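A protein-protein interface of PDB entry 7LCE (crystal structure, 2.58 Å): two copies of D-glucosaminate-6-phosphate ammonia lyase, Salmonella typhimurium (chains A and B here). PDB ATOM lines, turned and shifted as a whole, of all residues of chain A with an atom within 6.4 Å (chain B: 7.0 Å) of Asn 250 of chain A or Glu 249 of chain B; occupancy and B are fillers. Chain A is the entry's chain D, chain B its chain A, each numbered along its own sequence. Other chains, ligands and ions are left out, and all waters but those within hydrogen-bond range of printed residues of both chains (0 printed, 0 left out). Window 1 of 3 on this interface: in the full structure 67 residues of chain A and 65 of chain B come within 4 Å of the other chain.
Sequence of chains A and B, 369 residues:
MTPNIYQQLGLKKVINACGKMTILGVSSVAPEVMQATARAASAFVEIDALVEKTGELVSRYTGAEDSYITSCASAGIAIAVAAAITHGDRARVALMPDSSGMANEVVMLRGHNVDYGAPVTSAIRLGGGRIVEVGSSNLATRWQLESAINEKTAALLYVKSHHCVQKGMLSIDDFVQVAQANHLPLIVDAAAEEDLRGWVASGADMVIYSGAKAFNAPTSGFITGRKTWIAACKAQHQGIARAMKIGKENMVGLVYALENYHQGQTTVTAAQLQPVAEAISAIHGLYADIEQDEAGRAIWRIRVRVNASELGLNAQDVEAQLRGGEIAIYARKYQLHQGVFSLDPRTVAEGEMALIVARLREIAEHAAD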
ATOM      1  N   TYR A   6      -4.206  12.563  12.258  1.00  0.00           N
ATOM      2  CA  TYR A   6      -5.001  12.802  13.459  1.00  0.00           C
ATOM      3  C   TYR A   6      -6.485  12.599  13.181  1.00  0.00           C
ATOM      4  O   TYR A   6      -7.224  12.105  14.040  1.00  0.00           O
ATOM      5  CB  TYR A   6      -4.741  14.211  13.990  1.00  0.00           C
ATOM      6  CG  TYR A   6      -3.282  14.479  14.272  1.00  0.00           C
ATOM      7  CD1 TYR A   6      -2.615  13.799  15.280  1.00  0.00           C
ATOM      8  CD2 TYR A   6      -2.569  15.401  13.519  1.00  0.00           C
ATOM      9  CE1 TYR A   6      -1.279  14.035  15.537  1.00  0.00           C
ATOM     10  CE2 TYR A   6      -1.233  15.644  13.768  1.00  0.00           C
ATOM     11  CZ  TYR A   6      -0.593  14.959  14.777  1.00  0.00           C
ATOM     12  OH  TYR A   6       0.737  15.197  15.029  1.00  0.00           O
ATOM     13  N   GLY A  25       0.551  21.564  19.344  1.00  0.00           N
ATOM     14  CA  GLY A  25       1.693  20.852  18.815  1.00  0.00           C
ATOM     15  C   GLY A  25       2.881  21.714  18.457  1.00  0.00           C
ATOM     16  O   GLY A  25       3.787  21.226  17.771  1.00  0.00           O
ATOM     17  N   VAL A  29       6.454  20.511  11.102  1.00  0.00           N
ATOM     18  CA  VAL A  29       7.793  20.301  10.566  1.00  0.00           C
ATOM     19  C   VAL A  29       7.738  20.227   9.047  1.00  0.00           C
ATOM     20  O   VAL A  29       6.808  19.654   8.464  1.00  0.00           O
ATOM     21  CB  VAL A  29       8.419  19.030  11.163  1.00  0.00           C
ATOM     22  CG1 VAL A  29       9.869  18.902  10.726  1.00  0.00           C
ATOM     23  CG2 VAL A  29       8.316  19.049  12.679  1.00  0.00           C
ATOM     24  N   MET A  34      11.629  16.297   7.833  1.00  0.00           N
ATOM     25  CA  MET A  34      11.171  14.985   8.280  1.00  0.00           C
ATOM     26  C   MET A  34      11.789  13.862   7.458  1.00  0.00           C
ATOM     27  O   MET A  34      11.961  12.749   7.968  1.00  0.00           O
ATOM     28  CB  MET A  34       9.645  14.907   8.237  1.00  0.00           C
ATOM     29  CG  MET A  34       8.966  15.675   9.360  1.00  0.00           C
ATOM     30  SD  MET A  34       9.745  15.387  10.965  1.00  0.00           S
ATOM     31  CE  MET A  34       9.268  13.691  11.289  1.00  0.00           C
ATOM     32  N   THR A  37      14.889  13.334   9.189  1.00  0.00           N
ATOM     33  CA  THR A  37      14.610  12.700  10.474  1.00  0.00           C
ATOM     34  C   THR A  37      14.318  11.214  10.299  1.00  0.00           C
ATOM     35  O   THR A  37      14.779  10.387  11.096  1.00  0.00           O
ATOM     36  CB  THR A  37      13.441  13.403  11.162  1.00  0.00           C
ATOM     37  OG1 THR A  37      13.765  14.786  11.353  1.00  0.00           O
ATOM     38  CG2 THR A  37      13.142  12.761  12.512  1.00  0.00           C
ATOM     39  N   ALA A  40      17.461   9.303   9.665  1.00  0.00           N
ATOM     40  CA  ALA A  40      18.211   9.164  10.907  1.00  0.00           C
ATOM     41  C   ALA A  40      17.601   8.102  11.809  1.00  0.00           C
ATOM     42  O   ALA A  40      18.327   7.419  12.542  1.00  0.00           O
ATOM     43  CB  ALA A  40      18.275  10.505  11.636  1.00  0.00           C
ATOM     44  N   ILE A  69      22.474  19.582  22.086  1.00  0.00           N
ATOM     45  CA  ILE A  69      21.066  19.475  21.721  1.00  0.00           C
ATOM     46  C   ILE A  69      20.308  18.774  22.838  1.00  0.00           C
ATOM     47  O   ILE A  69      20.783  17.782  23.406  1.00  0.00           O
ATOM     48  CB  ILE A  69      20.909  18.737  20.377  1.00  0.00           C
ATOM     49  CG1 ILE A  69      21.570  19.539  19.254  1.00  0.00           C
ATOM     50  CG2 ILE A  69      19.446  18.488  20.062  1.00  0.00           C
ATOM     51  CD1 ILE A  69      21.322  18.982  17.868  1.00  0.00           C
ATOM     52  N   ALA A 217      11.010  22.715  13.862  1.00  0.00           N
ATOM     53  CA  ALA A 217      11.755  21.473  13.901  1.00  0.00           C
ATOM     54  C   ALA A 217      10.988  20.414  14.678  1.00  0.00           C
ATOM     55  O   ALA A 217      10.079  20.734  15.452  1.00  0.00           O
ATOM     56  CB  ALA A 217      13.123  21.692  14.563  1.00  0.00           C
ATOM     57  N   PRO A 218      11.319  19.136  14.494  1.00  0.00           N
ATOM     58  CA  PRO A 218      10.793  18.117  15.403  1.00  0.00           C
ATOM     59  C   PRO A 218      11.237  18.427  16.823  1.00  0.00           C
ATOM     60  O   PRO A 218      12.205  19.159  17.049  1.00  0.00           O
ATOM     61  CB  PRO A 218      11.410  16.814  14.883  1.00  0.00           C
ATOM     62  CG  PRO A 218      12.596  17.251  14.074  1.00  0.00           C
ATOM     63  CD  PRO A 218      12.174  18.544  13.451  1.00  0.00           C
ATOM     64  N   THR A 219      10.504  17.867  17.787  1.00  0.00           N
ATOM     65  CA  THR A 219      10.681  18.214  19.193  1.00  0.00           C
ATOM     66  C   THR A 219      12.148  18.201  19.597  1.00  0.00           C
ATOM     67  O   THR A 219      12.775  17.138  19.666  1.00  0.00           O
ATOM     68  CB  THR A 219       9.887  17.260  20.082  1.00  0.00           C
ATOM     69  OG1 THR A 219       8.521  17.252  19.655  1.00  0.00           O
ATOM     70  CG2 THR A 219       9.954  17.710  21.531  1.00  0.00           C
ATOM     71  N   SER A 220      12.703  19.383  19.847  1.00  0.00           N
ATOM     72  CA  SER A 220      14.129  19.525  20.102  1.00  0.00           C
ATOM     73  C   SER A 220      14.378  20.901  20.703  1.00  0.00           C
ATOM     74  O   SER A 220      13.529  21.795  20.644  1.00  0.00           O
ATOM     75  CB  SER A 220      14.951  19.343  18.826  1.00  0.00           C
ATOM     76  OG  SER A 220      14.599  20.314  17.856  1.00  0.00           O
ATOM     77  N   ILE A 246      16.360  13.096  23.984  1.00  0.00           N
ATOM     78  CA  ILE A 246      16.113  13.341  22.572  1.00  0.00           C
ATOM     79  C   ILE A 246      16.902  12.300  21.793  1.00  0.00           C
ATOM     80  O   ILE A 246      18.079  12.060  22.087  1.00  0.00           O
ATOM     81  CB  ILE A 246      16.501  14.770  22.150  1.00  0.00           C
ATOM     82  CG1 ILE A 246      16.342  14.933  20.637  1.00  0.00           C
ATOM     83  CG2 ILE A 246      17.916  15.108  22.595  1.00  0.00           C
ATOM     84  CD1 ILE A 246      16.536  16.341  20.146  1.00  0.00           C
ATOM     85  N   GLY A 247      16.250  11.660  20.830  1.00  0.00           N
ATOM     86  CA  GLY A 247      16.876  10.593  20.084  1.00  0.00           C
ATOM     87  C   GLY A 247      17.727  11.093  18.942  1.00  0.00           C
ATOM     88  O   GLY A 247      17.818  12.286  18.655  1.00  0.00           O
ATOM     89  N   LYS A 248      18.381  10.137  18.279  1.00  0.00           N
ATOM     90  CA  LYS A 248      19.207  10.475  17.127  1.00  0.00           C
ATOM     91  C   LYS A 248      18.372  11.063  15.997  1.00  0.00           C
ATOM     92  O   LYS A 248      18.877  11.875  15.212  1.00  0.00           O
ATOM     93  CB  LYS A 248      19.965   9.238  16.647  1.00  0.00           C
ATOM     94  CG  LYS A 248      19.091   8.004  16.492  1.00  0.00           C
ATOM     95  CD  LYS A 248      19.880   6.825  15.949  1.00  0.00           C
ATOM     96  CE  LYS A 248      19.015   5.577  15.848  1.00  0.00           C
ATOM     97  NZ  LYS A 248      17.723   5.832  15.153  1.00  0.00           N
ATOM     98  N   GLU A 249      17.096  10.676  15.901  1.00  0.00           N
ATOM     99  CA  GLU A 249      16.281  11.127  14.777  1.00  0.00           C
ATOM    100  C   GLU A 249      15.978  12.618  14.868  1.00  0.00           C
ATOM    101  O   GLU A 249      16.081  13.336  13.866  1.00  0.00           O
ATOM    102  CB  GLU A 249      14.994  10.297  14.678  1.00  0.00           C
ATOM    103  CG  GLU A 249      13.940  10.518  15.760  1.00  0.00           C
ATOM    104  CD  GLU A 249      14.283   9.838  17.071  1.00  0.00           C
ATOM    105  OE1 GLU A 249      15.261   9.062  17.097  1.00  0.00           O
ATOM    106  OE2 GLU A 249      13.560  10.063  18.066  1.00  0.00           O
ATOM    107  N   ASN A 250      15.625  13.111  16.056  1.00  0.00           N
ATOM    108  CA  ASN A 250      15.320  14.529  16.203  1.00  0.00           C
ATOM    109  C   ASN A 250      16.572  15.385  16.334  1.00  0.00           C
ATOM    110  O   ASN A 250      16.520  16.580  16.026  1.00  0.00           O
ATOM    111  CB  ASN A 250      14.411  14.755  17.412  1.00  0.00           C
ATOM    112  CG  ASN A 250      12.982  14.324  17.153  1.00  0.00           C
ATOM    113  OD1 ASN A 250      12.705  13.581  16.209  1.00  0.00           O
ATOM    114  ND2 ASN A 250      12.065  14.788  17.990  1.00  0.00           N
ATOM    115  N   MET A 251      17.688  14.804  16.781  1.00  0.00           N
ATOM    116  CA  MET A 251      18.963  15.511  16.725  1.00  0.00           C
ATOM    117  C   MET A 251      19.301  15.895  15.291  1.00  0.00           C
ATOM    118  O   MET A 251      19.658  17.046  15.010  1.00  0.00           O
ATOM    119  CB  MET A 251      20.068  14.646  17.329  1.00  0.00           C
ATOM    120  CG  MET A 251      20.031  14.570  18.843  1.00  0.00           C
ATOM    121  SD  MET A 251      21.264  13.430  19.496  1.00  0.00           S
ATOM    122  CE  MET A 251      22.779  14.285  19.069  1.00  0.00           C
ATOM    123  N   VAL A 252      19.197  14.938  14.370  1.00  0.00           N
ATOM    124  CA  VAL A 252      19.410  15.239  12.959  1.00  0.00           C
ATOM    125  C   VAL A 252      18.335  16.190  12.449  1.00  0.00           C
ATOM    126  O   VAL A 252      18.615  17.098  11.656  1.00  0.00           O
ATOM    127  CB  VAL A 252      19.456  13.935  12.143  1.00  0.00           C
ATOM    128  CG1 VAL A 252      19.522  14.232  10.656  1.00  0.00           C
ATOM    129  CG2 VAL A 252      20.645  13.093  12.572  1.00  0.00           C
ATOM    130  N   GLY A 253      17.092  16.005  12.903  1.00  0.00           N
ATOM    131  CA  GLY A 253      16.011  16.868  12.453  1.00  0.00           C
ATOM    132  C   GLY A 253      16.238  18.329  12.786  1.00  0.00           C
ATOM    133  O   GLY A 253      15.954  19.211  11.973  1.00  0.00           O
ATOM    134  N   LEU A 254      16.762  18.609  13.982  1.00  0.00           N
ATOM    135  CA  LEU A 254      17.036  19.996  14.349  1.00  0.00           C
ATOM    136  C   LEU A 254      18.090  20.610  13.435  1.00  0.00           C
ATOM    137  O   LEU A 254      17.953  21.762  13.005  1.00  0.00           O
ATOM    138  CB  LEU A 254      17.476  20.079  15.810  1.00  0.00           C
ATOM    139  CG  LEU A 254      18.010  21.446  16.245  1.00  0.00           C
ATOM    140  CD1 LEU A 254      16.933  22.519  16.134  1.00  0.00           C
ATOM    141  CD2 LEU A 254      18.568  21.383  17.656  1.00  0.00           C
ATOM    142  N   VAL A 255      19.145  19.853  13.121  1.00  0.00           N
ATOM    143  CA  VAL A 255      20.211  20.373  12.270  1.00  0.00           C
ATOM    144  C   VAL A 255      19.679  20.689  10.879  1.00  0.00           C
ATOM    145  O   VAL A 255      19.992  21.737  10.300  1.00  0.00           O
ATOM    146  CB  VAL A 255      21.384  19.377  12.211  1.00  0.00           C
ATOM    147  CG1 VAL A 255      22.470  19.896  11.285  1.00  0.00           C
ATOM    148  CG2 VAL A 255      21.938  19.129  13.602  1.00  0.00           C
ATOM    149  N   VAL B  33       6.566   3.213  10.114  1.00  0.00           N
ATOM    150  CA  VAL B  33       6.300   3.999  11.315  1.00  0.00           C
ATOM    151  C   VAL B  33       6.748   5.444  11.124  1.00  0.00           C
ATOM    152  O   VAL B  33       6.052   6.382  11.532  1.00  0.00           O
ATOM    153  CB  VAL B  33       6.971   3.345  12.535  1.00  0.00           C
ATOM    154  CG1 VAL B  33       6.708   4.156  13.787  1.00  0.00           C
ATOM    155  CG2 VAL B  33       6.460   1.927  12.714  1.00  0.00           C
ATOM    156  N   MET B  34       7.908   5.651  10.491  1.00  0.00           N
ATOM    157  CA  MET B  34       8.377   7.015  10.255  1.00  0.00           C
ATOM    158  C   MET B  34       7.482   7.754   9.268  1.00  0.00           C
ATOM    159  O   MET B  34       7.401   8.988   9.316  1.00  0.00           O
ATOM    160  CB  MET B  34       9.825   7.010   9.769  1.00  0.00           C
ATOM    161  CG  MET B  34      10.845   6.729  10.865  1.00  0.00           C
ATOM    162  SD  MET B  34      10.535   7.664  12.383  1.00  0.00           S
ATOM    163  CE  MET B  34      10.947   9.329  11.870  1.00  0.00           C
ATOM    164  N   ALA B  36       4.210   7.522   9.313  1.00  0.00           N
ATOM    165  CA  ALA B  36       3.176   8.039  10.201  1.00  0.00           C
ATOM    166  C   ALA B  36       3.711   9.167  11.072  1.00  0.00           C
ATOM    167  O   ALA B  36       2.987  10.124  11.373  1.00  0.00           O
ATOM    168  CB  ALA B  36       2.619   6.909  11.066  1.00  0.00           C
ATOM    169  N   THR B  37       4.980   9.076  11.478  1.00  0.00           N
ATOM    170  CA  THR B  37       5.576  10.133  12.289  1.00  0.00           C
ATOM    171  C   THR B  37       5.721  11.422  11.491  1.00  0.00           C
ATOM    172  O   THR B  37       5.461  12.514  12.013  1.00  0.00           O
ATOM    173  CB  THR B  37       6.936   9.678  12.824  1.00  0.00           C
ATOM    174  OG1 THR B  37       6.767   8.484  13.597  1.00  0.00           O
ATOM    175  CG2 THR B  37       7.559  10.757  13.698  1.00  0.00           C
ATOM    176  N   ALA B  38       6.133  11.315  10.225  1.00  0.00           N
ATOM    177  CA  ALA B  38       6.295  12.502   9.393  1.00  0.00           C
ATOM    178  C   ALA B  38       4.958  13.186   9.135  1.00  0.00           C
ATOM    179  O   ALA B  38       4.866  14.419   9.181  1.00  0.00           O
ATOM    180  CB  ALA B  38       6.974  12.132   8.075  1.00  0.00           C
ATOM    181  N   ARG B  39       3.911  12.406   8.854  1.00  0.00           N
ATOM    182  CA  ARG B  39       2.592  12.998   8.664  1.00  0.00           C
ATOM    183  C   ARG B  39       2.108  13.664   9.943  1.00  0.00           C
ATOM    184  O   ARG B  39       1.454  14.713   9.899  1.00  0.00           O
ATOM    185  CB  ARG B  39       1.594  11.938   8.188  1.00  0.00           C
ATOM    186  CG  ARG B  39       1.920  11.375   6.810  1.00  0.00           C
ATOM    187  CD  ARG B  39       0.966  10.266   6.385  1.00  0.00           C
ATOM    188  NE  ARG B  39      -0.426  10.700   6.388  1.00  0.00           N
ATOM    189  CZ  ARG B  39      -1.392  10.126   7.093  1.00  0.00           C
ATOM    190  NH1 ARG B  39      -1.160   9.063   7.844  1.00  0.00           N
ATOM    191  NH2 ARG B  39      -2.623  10.625   7.031  1.00  0.00           N
ATOM    192  N   ALA B  40       2.441  13.081  11.096  1.00  0.00           N
ATOM    193  CA  ALA B  40       2.064  13.693  12.365  1.00  0.00           C
ATOM    194  C   ALA B  40       2.829  14.985  12.611  1.00  0.00           C
ATOM    195  O   ALA B  40       2.284  15.927  13.197  1.00  0.00           O
ATOM    196  CB  ALA B  40       2.303  12.714  13.513  1.00  0.00           C
ATOM    197  N   ALA B  41       4.089  15.049  12.174  1.00  0.00           N
ATOM    198  CA  ALA B  41       4.884  16.255  12.370  1.00  0.00           C
ATOM    199  C   ALA B  41       4.412  17.394  11.474  1.00  0.00           C
ATOM    200  O   ALA B  41       4.588  18.567  11.821  1.00  0.00           O
ATOM    201  CB  ALA B  41       6.360  15.956  12.116  1.00  0.00           C
ATOM    202  N   SER B  42       3.834  17.073  10.319  1.00  0.00           N
ATOM    203  CA  SER B  42       3.440  18.069   9.334  1.00  0.00           C
ATOM    204  C   SER B  42       2.027  18.605   9.552  1.00  0.00           C
ATOM    205  O   SER B  42       1.472  19.235   8.645  1.00  0.00           O
ATOM    206  CB  SER B  42       3.564  17.484   7.926  1.00  0.00           C
ATOM    207  OG  SER B  42       4.898  17.088   7.656  1.00  0.00           O
ATOM    208  N   LEU B  50      -5.091  14.485  21.813  1.00  0.00           N
ATOM    209  CA  LEU B  50      -4.093  13.505  21.398  1.00  0.00           C
ATOM    210  C   LEU B  50      -3.559  12.719  22.589  1.00  0.00           C
ATOM    211  O   LEU B  50      -3.327  11.510  22.487  1.00  0.00           O
ATOM    212  CB  LEU B  50      -2.955  14.203  20.657  1.00  0.00           C
ATOM    213  CG  LEU B  50      -1.883  13.274  20.089  1.00  0.00           C
ATOM    214  CD1 LEU B  50      -2.478  12.333  19.056  1.00  0.00           C
ATOM    215  CD2 LEU B  50      -0.750  14.086  19.498  1.00  0.00           C
ATOM    216  N   PRO B 218      10.278   5.419  17.494  1.00  0.00           N
ATOM    217  CA  PRO B 218      10.977   6.680  17.741  1.00  0.00           C
ATOM    218  C   PRO B 218      11.006   6.962  19.235  1.00  0.00           C
ATOM    219  O   PRO B 218      10.209   6.421  20.006  1.00  0.00           O
ATOM    220  CB  PRO B 218      10.135   7.714  16.980  1.00  0.00           C
ATOM    221  CG  PRO B 218       8.807   7.068  16.805  1.00  0.00           C
ATOM    222  CD  PRO B 218       9.108   5.612  16.622  1.00  0.00           C
ATOM    223  N   THR B 219      11.951   7.811  19.640  1.00  0.00           N
ATOM    224  CA  THR B 219      12.240   8.052  21.050  1.00  0.00           C
ATOM    225  C   THR B 219      10.972   8.300  21.854  1.00  0.00           C
ATOM    226  O   THR B 219      10.341   9.354  21.722  1.00  0.00           O
ATOM    227  CB  THR B 219      13.185   9.238  21.193  1.00  0.00           C
ATOM    228  OG1 THR B 219      14.340   9.003  20.383  1.00  0.00           O
ATOM    229  CG2 THR B 219      13.607   9.403  22.642  1.00  0.00           C
ATOM    230  N   ILE B 246       7.855  14.866  24.982  1.00  0.00           N
ATOM    231  CA  ILE B 246       7.739  14.120  23.737  1.00  0.00           C
ATOM    232  C   ILE B 246       6.677  14.811  22.894  1.00  0.00           C
ATOM    233  O   ILE B 246       5.596  15.142  23.396  1.00  0.00           O
ATOM    234  CB  ILE B 246       7.399  12.634  23.975  1.00  0.00           C
ATOM    235  CG1 ILE B 246       7.178  11.916  22.641  1.00  0.00           C
ATOM    236  CG2 ILE B 246       6.186  12.473  24.883  1.00  0.00           C
ATOM    237  CD1 ILE B 246       7.003  10.422  22.775  1.00  0.00           C
ATOM    238  N   GLY B 247       6.991  15.049  21.624  1.00  0.00           N
ATOM    239  CA  GLY B 247       6.099  15.783  20.755  1.00  0.00           C
ATOM    240  C   GLY B 247       5.014  14.919  20.153  1.00  0.00           C
ATOM    241  O   GLY B 247       4.947  13.706  20.355  1.00  0.00           O
ATOM    242  N   LYS B 248       4.133  15.578  19.398  1.00  0.00           N
ATOM    243  CA  LYS B 248       3.047  14.870  18.729  1.00  0.00           C
ATOM    244  C   LYS B 248       3.569  13.866  17.712  1.00  0.00           C
ATOM    245  O   LYS B 248       2.919  12.844  17.458  1.00  0.00           O
ATOM    246  CB  LYS B 248       2.108  15.868  18.052  1.00  0.00           C
ATOM    247  CG  LYS B 248       2.821  16.920  17.216  1.00  0.00           C
ATOM    248  CD  LYS B 248       1.836  17.845  16.521  1.00  0.00           C
ATOM    249  CE  LYS B 248       2.558  18.936  15.742  1.00  0.00           C
ATOM    250  NZ  LYS B 248       3.630  18.395  14.863  1.00  0.00           N
ATOM    251  N   GLU B 249       4.737  14.129  17.123  1.00  0.00           N
ATOM    252  CA  GLU B 249       5.238  13.251  16.072  1.00  0.00           C
ATOM    253  C   GLU B 249       5.643  11.890  16.633  1.00  0.00           C
ATOM    254  O   GLU B 249       5.318  10.852  16.045  1.00  0.00           O
ATOM    255  CB  GLU B 249       6.401  13.921  15.330  1.00  0.00           C
ATOM    256  CG  GLU B 249       7.711  14.052  16.104  1.00  0.00           C
ATOM    257  CD  GLU B 249       7.690  15.165  17.134  1.00  0.00           C
ATOM    258  OE1 GLU B 249       6.727  15.961  17.143  1.00  0.00           O
ATOM    259  OE2 GLU B 249       8.642  15.245  17.938  1.00  0.00           O
ATOM    260  N   ASN B 250       6.338  11.872  17.772  1.00  0.00           N
ATOM    261  CA  ASN B 250       6.757  10.611  18.373  1.00  0.00           C
ATOM    262  C   ASN B 250       5.655   9.957  19.196  1.00  0.00           C
ATOM    263  O   ASN B 250       5.684   8.735  19.381  1.00  0.00           O
ATOM    264  CB  ASN B 250       8.004  10.828  19.233  1.00  0.00           C
ATOM    265  CG  ASN B 250       9.257  11.017  18.398  1.00  0.00           C
ATOM    266  OD1 ASN B 250       9.183  11.289  17.199  1.00  0.00           O
ATOM    267  ND2 ASN B 250      10.417  10.878  19.029  1.00  0.00           N
ATOM    268  N   MET B 251       4.690  10.733  19.694  1.00  0.00           N
ATOM    269  CA  MET B 251       3.499  10.133  20.284  1.00  0.00           C
ATOM    270  C   MET B 251       2.784   9.256  19.266  1.00  0.00           C
ATOM    271  O   MET B 251       2.457   8.097  19.545  1.00  0.00           O
ATOM    272  CB  MET B 251       2.562  11.221  20.808  1.00  0.00           C
ATOM    273  CG  MET B 251       3.012  11.869  22.099  1.00  0.00           C
ATOM    274  SD  MET B 251       1.945  13.242  22.579  1.00  0.00           S
ATOM    275  CE  MET B 251       0.415  12.384  22.948  1.00  0.00           C
ATOM    276  N   VAL B 252       2.549   9.794  18.068  1.00  0.00           N
ATOM    277  CA  VAL B 252       1.942   9.009  16.998  1.00  0.00           C
ATOM    278  C   VAL B 252       2.870   7.876  16.579  1.00  0.00           C
ATOM    279  O   VAL B 252       2.422   6.761  16.282  1.00  0.00           O
ATOM    280  CB  VAL B 252       1.584   9.922  15.809  1.00  0.00           C
ATOM    281  CG1 VAL B 252       1.082   9.102  14.632  1.00  0.00           C
ATOM    282  CG2 VAL B 252       0.551  10.954  16.228  1.00  0.00           C
ATOM    283  N   GLY B 253       4.178   8.144  16.553  1.00  0.00           N
ATOM    284  CA  GLY B 253       5.127   7.118  16.154  1.00  0.00           C
ATOM    285  C   GLY B 253       5.080   5.892  17.046  1.00  0.00           C
ATOM    286  O   GLY B 253       5.159   4.760  16.563  1.00  0.00           O
ATOM    287  N   LEU B 254       4.938   6.098  18.357  1.00  0.00           N
ATOM    288  CA  LEU B 254       4.853   4.966  19.275  1.00  0.00           C
ATOM    289  C   LEU B 254       3.617   4.119  18.998  1.00  0.00           C
ATOM    290  O   LEU B 254       3.684   2.884  19.011  1.00  0.00           O
ATOM    291  CB  LEU B 254       4.848   5.460  20.721  1.00  0.00           C
ATOM    292  CG  LEU B 254       4.536   4.398  21.779  1.00  0.00           C
ATOM    293  CD1 LEU B 254       5.600   3.311  21.785  1.00  0.00           C
ATOM    294  CD2 LEU B 254       4.390   5.027  23.155  1.00  0.00           C
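Asn 250 of chain A touches just one residue of chain B: Glu 249 (3.5 Å).
Glu 249 of chain B touches just these residues of chain A: Thr 219 (2.6 Å) and Asn 250 (3.5 Å).
Of the printed residues of chain B, Tyr 6 of chain A touches Ala 40 (2.5 Å), Leu 50 (3.996 Å), Lys 248 (3.2 Å) and Val 252 (3.6 Å).
Of the printed residues of chain A, Ser 42 of chain B touches Val 29 (3.3 Å).
Of the printed residues of chain B, Glu 249 of chain A touches Thr 219 and Asn 250.
Ile 246 of chain B touches none of the printed residues of chain A.
The nearest residue of chain A that does not touch Glu 249 of chain B is Pro 218 of chain A (4.3 Å).
The nearest printed residue of chain B that does not touch Gly 25 of chain A is Glu 249 of chain B (6.1 Å).
Thr 219 of chain A touches Glu 249 of chain B, and with the chains exchanged Glu 249 of chain A touches Thr 219 of chain B.
Glu 249 of chain A touches Asn 250 of chain B, and with the chains exchanged Asn 250 of chain A touches Glu 249 of chain B.
Positions printed for both chains: 34, 37, 40, 218, 219, 246, 247, 248, 249, 250, 251, 252, 253 and 254.
Hydrophobic or aromatic side chains of chain B within 4 Å of the printed part of chain A: Ala 38, Ala 40, Ala 41, Leu 50 and Val 252.
Of the 21 printed residues of chain A, 8 touch a printed residue of chain B.
Hydrophobic or aromatic side chains of chain A that line the printed part of chain B: Tyr 6, Val 29 and Met 34.
Along chain A the printed residues that touch a printed residue of chain B span positions 6 to 250.
NZ of Lys 248 of chain B is in hydrogen-bond range of O of Ala 41 of chain B (3.2 Å).
The side-chain hydroxyl of Ser 42 of chain B is in hydrogen-bond range of the backbone carbonyl oxygen of Ala 38 of chain B, at 3.1 Å.
ND2 of Asn 250 of chain B lies within hydrogen-bond range of O of Thr 219 of chain B (3.1 Å).
The backbone carbonyl oxygen (O) of Ala 41 of chain B is in hydrogen-bond range of the backbone NH (N) of Val 29 of chain A (2.8 Å).
The side-chain carboxylate (OE2) of Glu 249 of chain A lies within hydrogen-bond range of the side-chain amide nitrogen (ND2) of Asn 250 of chain B, at 3.4 Å.
The side-chain hydroxyl (OG1) of Thr 219 of chain A sits close to the backbone NH (N) of Gly 247 of chain B.
The side-chain hydroxyl of Thr 219 of chain B lies within hydrogen-bond range of the side-chain carboxylate of Glu 249 of chain A (2.7 Å).
The side-chain hydroxyl (OG) of Ser 42 of chain B sits at hydrogen-bond distance from the backbone carbonyl oxygen (O) of Val 29 of chain A, at 3.3 Å.
OG1 of Thr 219 of chain B sits close to N of Gly 247 of chain A, at 3.3 Å.
The side-chain amide nitrogen (ND2) of Asn 250 of chain A is in hydrogen-bond range of the side-chain carboxylate (OE2) of Glu 249 of chain B (3.5 Å).
The side-chain hydroxyl (OG1) of Thr 219 of chain A lies within hydrogen-bond range of the side-chain carboxylate (OE2) of Glu 249 of chain B, 2.6 Å away.
The backbone carbonyl oxygen of Ala 40 of chain B is in hydrogen-bond range of the side-chain hydroxyl of Tyr 6 of chain A, at 2.5 Å.
Among the printed residues, merely in contact across the chains: Tyr 6 of chain A with Leu 50 of chain B (3.996 Å), Tyr 6 of chain A with Lys 248 of chain B (3.2 Å), Tyr 6 of chain A with Val 252 of chain B (3.6 Å), Gly 25 of chain A with Lys 248 of chain B (3.3 Å), Met 34 of chain A with Ala 38 of chain B (3.7 Å) and Met 34 of chain A with Ala 41 of chain B (3.6 Å).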
